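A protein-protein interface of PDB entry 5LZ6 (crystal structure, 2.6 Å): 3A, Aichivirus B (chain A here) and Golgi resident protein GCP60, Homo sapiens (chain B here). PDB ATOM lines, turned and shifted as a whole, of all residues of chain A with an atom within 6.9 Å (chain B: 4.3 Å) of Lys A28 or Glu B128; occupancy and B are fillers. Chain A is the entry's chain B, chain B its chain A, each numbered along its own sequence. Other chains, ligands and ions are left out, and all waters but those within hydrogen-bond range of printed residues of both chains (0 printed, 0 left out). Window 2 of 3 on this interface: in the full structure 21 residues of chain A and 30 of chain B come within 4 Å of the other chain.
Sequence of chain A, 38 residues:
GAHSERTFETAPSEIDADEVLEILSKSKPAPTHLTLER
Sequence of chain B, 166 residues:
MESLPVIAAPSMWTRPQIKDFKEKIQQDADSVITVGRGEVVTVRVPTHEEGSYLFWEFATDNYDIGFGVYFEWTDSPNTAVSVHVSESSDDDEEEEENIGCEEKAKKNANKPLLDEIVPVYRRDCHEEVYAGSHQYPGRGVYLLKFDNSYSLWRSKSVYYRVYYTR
OE2 of Glu B128 lies within salt-bridge range of NZ of Lys A28 (3.9 Å).
The backbone carbonyl oxygen of Lys A28 is in hydrogen-bond range of the backbone NH of Thr B14, at 2.8 Å.
O of Arg B15 sits at hydrogen-bond distance from N of Val B129 (2.7 Å).
The side-chain hydroxyl of Ser A27 is in hydrogen-bond range of the backbone carbonyl oxygen of Ile A23.
Among the printed residues, pairs that only touch across the chains: Ile A23 with Arg B15 (3.3 Å), Leu A24 with Trp B13 (3.4 Å), Lys A26 with Arg B15 (3.6 Å), Ser A27 with Trp B13 (3.6 Å), Ser A27 with Thr B14 (3.2 Å), Ser A27 with Arg B15 (3.5 Å), Lys A28 with Trp B13 (3.2 Å), Pro A29 with Trp B13 (3.8 Å), Ala A30 with Trp B13 (3.9 Å) and Ala A30 with Thr B14 (3.9 Å).
Of the printed residues of chain B, Ile A23 touches Arg B15 (3.3 Å).
Of the printed residues of chain B, Lys A26 touches Arg B15 (3.6 Å).
Printed residues of chain B within 4 Å of Ser A27: Trp B13 (3.6 Å), Thr B14 (3.2 Å) and Arg B15 (3.5 Å).
Lys A28 touches just these residues of chain B: Trp B13 (3.2 Å), Thr B14 (2.8 Å) and Glu B128 (3.9 Å).
Printed residues of chain A within 4 Å of Thr B14: Ser A27, Lys A28 and Ala A30.
Printed residues of chain A within 4 Å of Arg B15: Ile A23 (3.3 Å), Lys A26 (3.6 Å) and Ser A27 (3.5 Å).
His B126 touches none of the printed residues of chain A.
Of chain A, only Lys A28 comes within 4 Å of Glu B128.
The nearest printed residue of chain B that does not touch Pro A29 is Thr B14 (4.5 Å).
Hydrophobic or aromatic side chains of chain B within 4 Å of the printed part of chain A: Trp B13.
Along chain A the printed residues that touch a printed residue of chain B span positions 23 to 30.
Among the printed residues, Asp or Glu carboxylates within 4 Å of a Lys or Arg side-chain nitrogen of the other chain: Lys A28 with Glu B128.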
ATOM      1  N   ILE A  23      14.100  -2.764   5.901  1.00  0.00           N
ATOM      2  CA  ILE A  23      14.268  -1.328   6.099  1.00  0.00           C
ATOM      3  C   ILE A  23      14.044  -0.563   4.798  1.00  0.00           C
ATOM      4  O   ILE A  23      13.234   0.362   4.746  1.00  0.00           O
ATOM      5  CB  ILE A  23      15.678  -1.002   6.655  1.00  0.00           C
ATOM      6  CG1 ILE A  23      15.831  -1.577   8.064  1.00  0.00           C
ATOM      7  CG2 ILE A  23      15.922   0.504   6.692  1.00  0.00           C
ATOM      8  CD1 ILE A  23      17.235  -1.477   8.637  1.00  0.00           C
ATOM      9  N   LEU A  24      14.762  -0.953   3.751  1.00  0.00           N
ATOM     10  CA  LEU A  24      14.785  -0.181   2.513  1.00  0.00           C
ATOM     11  C   LEU A  24      13.497  -0.321   1.701  1.00  0.00           C
ATOM     12  O   LEU A  24      13.215   0.507   0.836  1.00  0.00           O
ATOM     13  CB  LEU A  24      15.985  -0.596   1.659  1.00  0.00           C
ATOM     14  CG  LEU A  24      17.367  -0.307   2.256  1.00  0.00           C
ATOM     15  CD1 LEU A  24      18.462  -0.838   1.345  1.00  0.00           C
ATOM     16  CD2 LEU A  24      17.574   1.182   2.510  1.00  0.00           C
ATOM     17  N   SER A  25      12.717  -1.362   1.976  1.00  0.00           N
ATOM     18  CA  SER A  25      11.440  -1.547   1.291  1.00  0.00           C
ATOM     19  C   SER A  25      10.471  -0.421   1.633  1.00  0.00           C
ATOM     20  O   SER A  25       9.518  -0.166   0.894  1.00  0.00           O
ATOM     21  CB  SER A  25      10.819  -2.895   1.659  1.00  0.00           C
ATOM     22  OG  SER A  25      10.648  -3.011   3.059  1.00  0.00           O
ATOM     23  N   LYS A  26      10.724   0.247   2.755  1.00  0.00           N
ATOM     24  CA  LYS A  26       9.869   1.329   3.229  1.00  0.00           C
ATOM     25  C   LYS A  26      10.484   2.695   2.945  1.00  0.00           C
ATOM     26  O   LYS A  26       9.822   3.723   3.092  1.00  0.00           O
ATOM     27  CB  LYS A  26       9.616   1.187   4.734  1.00  0.00           C
ATOM     28  CG  LYS A  26       9.258  -0.219   5.187  1.00  0.00           C
ATOM     29  CD  LYS A  26       9.203  -0.303   6.704  1.00  0.00           C
ATOM     30  CE  LYS A  26       8.894  -1.714   7.178  1.00  0.00           C
ATOM     31  NZ  LYS A  26       8.977  -1.833   8.660  1.00  0.00           N
ATOM     32  N   SER A  27      11.748   2.702   2.531  1.00  0.00           N
ATOM     33  CA  SER A  27      12.520   3.940   2.456  1.00  0.00           C
ATOM     34  C   SER A  27      12.643   4.472   1.031  1.00  0.00           C
ATOM     35  O   SER A  27      12.512   3.723   0.066  1.00  0.00           O
ATOM     36  CB  SER A  27      13.919   3.722   3.041  1.00  0.00           C
ATOM     37  OG  SER A  27      13.860   3.001   4.259  1.00  0.00           O
ATOM     38  N   LYS A  28      12.889   5.775   0.919  1.00  0.00           N
ATOM     39  CA  LYS A  28      13.181   6.412  -0.363  1.00  0.00           C
ATOM     40  C   LYS A  28      14.505   7.174  -0.271  1.00  0.00           C
ATOM     41  O   LYS A  28      14.905   7.587   0.817  1.00  0.00           O
ATOM     42  CB  LYS A  28      12.047   7.354  -0.775  1.00  0.00           C
ATOM     43  CG  LYS A  28      11.683   8.395   0.272  1.00  0.00           C
ATOM     44  CD  LYS A  28      10.521   9.261  -0.193  1.00  0.00           C
ATOM     45  CE  LYS A  28      10.080  10.241   0.886  1.00  0.00           C
ATOM     46  NZ  LYS A  28      11.133  11.245   1.213  1.00  0.00           N
ATOM     47  N   PRO A  29      15.191   7.361  -1.412  1.00  0.00           N
ATOM     48  CA  PRO A  29      16.505   8.019  -1.416  1.00  0.00           C
ATOM     49  C   PRO A  29      16.498   9.409  -0.788  1.00  0.00           C
ATOM     50  O   PRO A  29      15.515  10.138  -0.921  1.00  0.00           O
ATOM     51  CB  PRO A  29      16.848   8.114  -2.905  1.00  0.00           C
ATOM     52  CG  PRO A  29      16.067   7.035  -3.547  1.00  0.00           C
ATOM     53  CD  PRO A  29      14.793   6.933  -2.766  1.00  0.00           C
ATOM     54  N   ALA A  30      17.593   9.755  -0.117  1.00  0.00           N
ATOM     55  CA  ALA A  30      17.770  11.079   0.468  1.00  0.00           C
ATOM     56  C   ALA A  30      19.108  11.661   0.026  1.00  0.00           C
ATOM     57  O   ALA A  30      20.025  10.912  -0.317  1.00  0.00           O
ATOM     58  CB  ALA A  30      17.695  11.008   1.982  1.00  0.00           C
ATOM     59  N   TRP B  13      18.841   7.087   2.839  1.00  0.00           N
ATOM     60  CA  TRP B  13      17.410   6.935   2.629  1.00  0.00           C
ATOM     61  C   TRP B  13      16.621   7.539   3.782  1.00  0.00           C
ATOM     62  O   TRP B  13      17.185   7.862   4.829  1.00  0.00           O
ATOM     63  CB  TRP B  13      17.048   5.457   2.479  1.00  0.00           C
ATOM     64  CG  TRP B  13      17.754   4.755   1.361  1.00  0.00           C
ATOM     65  CD1 TRP B  13      17.334   4.651   0.068  1.00  0.00           C
ATOM     66  CD2 TRP B  13      18.999   4.048   1.436  1.00  0.00           C
ATOM     67  NE1 TRP B  13      18.240   3.926  -0.668  1.00  0.00           N
ATOM     68  CE2 TRP B  13      19.272   3.544   0.147  1.00  0.00           C
ATOM     69  CE3 TRP B  13      19.910   3.791   2.465  1.00  0.00           C
ATOM     70  CZ2 TRP B  13      20.416   2.801  -0.139  1.00  0.00           C
ATOM     71  CZ3 TRP B  13      21.048   3.053   2.177  1.00  0.00           C
ATOM     72  CH2 TRP B  13      21.289   2.567   0.886  1.00  0.00           C
ATOM     73  N   THR B  14      15.314   7.688   3.580  1.00  0.00           N
ATOM     74  CA  THR B  14      14.414   8.128   4.637  1.00  0.00           C
ATOM     75  C   THR B  14      13.132   7.306   4.623  1.00  0.00           C
ATOM     76  O   THR B  14      12.635   6.947   3.556  1.00  0.00           O
ATOM     77  CB  THR B  14      14.053   9.618   4.499  1.00  0.00           C
ATOM     78  OG1 THR B  14      13.685   9.899   3.143  1.00  0.00           O
ATOM     79  CG2 THR B  14      15.230  10.500   4.902  1.00  0.00           C
ATOM     80  N   ARG B  15      12.609   7.000   5.809  1.00  0.00           N
ATOM     81  CA  ARG B  15      11.318   6.326   5.926  1.00  0.00           C
ATOM     82  C   ARG B  15      10.501   6.915   7.082  1.00  0.00           C
ATOM     83  O   ARG B  15      11.059   7.258   8.124  1.00  0.00           O
ATOM     84  CB  ARG B  15      11.508   4.817   6.118  1.00  0.00           C
ATOM     85  CG  ARG B  15      11.962   4.386   7.506  1.00  0.00           C
ATOM     86  CD  ARG B  15      12.044   2.870   7.589  1.00  0.00           C
ATOM     87  NE  ARG B  15      12.393   2.397   8.927  1.00  0.00           N
ATOM     88  CZ  ARG B  15      13.629   2.357   9.412  1.00  0.00           C
ATOM     89  NH1 ARG B  15      14.653   2.774   8.679  1.00  0.00           N
ATOM     90  NH2 ARG B  15      13.843   1.904  10.639  1.00  0.00           N
ATOM     91  N   PRO B  16       9.173   7.038   6.896  1.00  0.00           N
ATOM     92  CA  PRO B  16       8.299   7.684   7.886  1.00  0.00           C
ATOM     93  C   PRO B  16       7.928   6.826   9.099  1.00  0.00           C
ATOM     94  O   PRO B  16       7.303   7.342  10.025  1.00  0.00           O
ATOM     95  CB  PRO B  16       7.043   8.004   7.074  1.00  0.00           C
ATOM     96  CG  PRO B  16       7.013   6.967   6.014  1.00  0.00           C
ATOM     97  CD  PRO B  16       8.446   6.732   5.649  1.00  0.00           C
ATOM     98  N   ILE B  18       8.625   6.139  11.971  1.00  0.00           N
ATOM     99  CA  ILE B  18       9.523   6.648  12.999  1.00  0.00           C
ATOM    100  C   ILE B  18       9.151   6.184  14.407  1.00  0.00           C
ATOM    101  O   ILE B  18      10.024   5.991  15.252  1.00  0.00           O
ATOM    102  CB  ILE B  18       9.565   8.197  12.966  1.00  0.00           C
ATOM    103  CG1 ILE B  18      10.579   8.733  13.977  1.00  0.00           C
ATOM    104  CG2 ILE B  18       8.185   8.788  13.236  1.00  0.00           C
ATOM    105  CD1 ILE B  18      10.976  10.180  13.728  1.00  0.00           C
ATOM    106  N   ALA B  59      17.299   8.810  14.291  1.00  0.00           N
ATOM    107  CA  ALA B  59      16.148   9.706  14.346  1.00  0.00           C
ATOM    108  C   ALA B  59      16.173  10.516  15.639  1.00  0.00           C
ATOM    109  O   ALA B  59      16.856  10.142  16.594  1.00  0.00           O
ATOM    110  CB  ALA B  59      14.850   8.917  14.236  1.00  0.00           C
ATOM    111  N   ASP B 124      16.153  16.616   8.824  1.00  0.00           N
ATOM    112  CA  ASP B 124      14.847  16.550   9.464  1.00  0.00           C
ATOM    113  C   ASP B 124      14.542  15.123   9.895  1.00  0.00           C
ATOM    114  O   ASP B 124      13.585  14.509   9.426  1.00  0.00           O
ATOM    115  CB  ASP B 124      13.762  17.068   8.523  1.00  0.00           C
ATOM    116  CG  ASP B 124      13.861  18.560   8.290  1.00  0.00           C
ATOM    117  OD1 ASP B 124      14.346  19.271   9.195  1.00  0.00           O
ATOM    118  OD2 ASP B 124      13.459  19.025   7.203  1.00  0.00           O
ATOM    119  N   CYS B 125      15.371  14.605  10.794  1.00  0.00           N
ATOM    120  CA  CYS B 125      15.242  13.231  11.261  1.00  0.00           C
ATOM    121  C   CYS B 125      14.302  13.130  12.461  1.00  0.00           C
ATOM    122  O   CYS B 125      14.237  12.098  13.128  1.00  0.00           O
ATOM    123  CB  CYS B 125      16.618  12.663  11.612  1.00  0.00           C
ATOM    124  SG  CYS B 125      17.619  13.714  12.691  1.00  0.00           S
ATOM    125  N   HIS B 126      13.575  14.210  12.727  1.00  0.00           N
ATOM    126  CA  HIS B 126      12.526  14.205  13.742  1.00  0.00           C
ATOM    127  C   HIS B 126      11.182  13.898  13.093  1.00  0.00           C
ATOM    128  O   HIS B 126      10.220  13.542  13.776  1.00  0.00           O
ATOM    129  CB  HIS B 126      12.467  15.546  14.485  1.00  0.00           C
ATOM    130  CG  HIS B 126      12.268  16.736  13.595  1.00  0.00           C
ATOM    131  ND1 HIS B 126      13.152  17.080  12.596  1.00  0.00           N
ATOM    132  CD2 HIS B 126      11.293  17.676  13.572  1.00  0.00           C
ATOM    133  CE1 HIS B 126      12.724  18.170  11.985  1.00  0.00           C
ATOM    134  NE2 HIS B 126      11.599  18.553  12.560  1.00  0.00           N
ATOM    135  N   GLU B 127      11.132  14.034  11.770  1.00  0.00           N
ATOM    136  CA  GLU B 127       9.927  13.760  10.996  1.00  0.00           C
ATOM    137  C   GLU B 127       9.993  12.379  10.345  1.00  0.00           C
ATOM    138  O   GLU B 127       8.971  11.719  10.164  1.00  0.00           O
ATOM    139  CB  GLU B 127       9.733  14.841   9.930  1.00  0.00           C
ATOM    140  CG  GLU B 127       9.577  16.247  10.506  1.00  0.00           C
ATOM    141  CD  GLU B 127       9.646  17.337   9.449  1.00  0.00           C
ATOM    142  OE1 GLU B 127       9.992  17.032   8.288  1.00  0.00           O
ATOM    143  OE2 GLU B 127       9.354  18.505   9.782  1.00  0.00           O
ATOM    144  N   GLU B 128      11.205  11.954   9.997  1.00  0.00           N
ATOM    145  CA  GLU B 128      11.427  10.655   9.365  1.00  0.00           C
ATOM    146  C   GLU B 128      12.673   9.979   9.930  1.00  0.00           C
ATOM    147  O   GLU B 128      13.470  10.613  10.622  1.00  0.00           O
ATOM    148  CB  GLU B 128      11.566  10.813   7.850  1.00  0.00           C
ATOM    149  CG  GLU B 128      10.296  11.267   7.146  1.00  0.00           C
ATOM    150  CD  GLU B 128      10.519  11.567   5.676  1.00  0.00           C
ATOM    151  OE1 GLU B 128      11.591  12.108   5.332  1.00  0.00           O
ATOM    152  OE2 GLU B 128       9.622  11.259   4.862  1.00  0.00           O
ATOM    153  N   VAL B 129      12.834   8.694   9.631  1.00  0.00           N
ATOM    154  CA  VAL B 129      14.032   7.958  10.019  1.00  0.00           C
ATOM    155  C   VAL B 129      15.032   7.974   8.875  1.00  0.00           C
ATOM    156  O   VAL B 129      14.716   7.544   7.770  1.00  0.00           O
ATOM    157  CB  VAL B 129      13.719   6.494  10.392  1.00  0.00           C
ATOM    158  CG1 VAL B 129      14.987   5.764  10.827  1.00  0.00           C
ATOM    159  CG2 VAL B 129      12.678   6.436  11.490  1.00  0.00           C
ATOM    160  N   TYR B 130      16.236   8.468   9.145  1.00  0.00           N
ATOM    161  CA  TYR B 130      17.303   8.470   8.152  1.00  0.00           C
ATOM    162  C   TYR B 130      18.158   7.216   8.257  1.00  0.00           C
ATOM    163  O   TYR B 130      18.732   6.933   9.309  1.00  0.00           O
ATOM    164  CB  TYR B 130      18.183   9.711   8.313  1.00  0.00           C
ATOM    165  CG  TYR B 130      17.555  10.965   7.759  1.00  0.00           C
ATOM    166  CD1 TYR B 130      16.397  11.489   8.316  1.00  0.00           C
ATOM    167  CD2 TYR B 130      18.117  11.623   6.676  1.00  0.00           C
ATOM    168  CE1 TYR B 130      15.818  12.633   7.810  1.00  0.00           C
ATOM    169  CE2 TYR B 130      17.546  12.768   6.162  1.00  0.00           C
ATOM    170  CZ  TYR B 130      16.397  13.268   6.734  1.00  0.00           C
ATOM    171  OH  TYR B 130      15.823  14.410   6.225  1.00  0.00           O
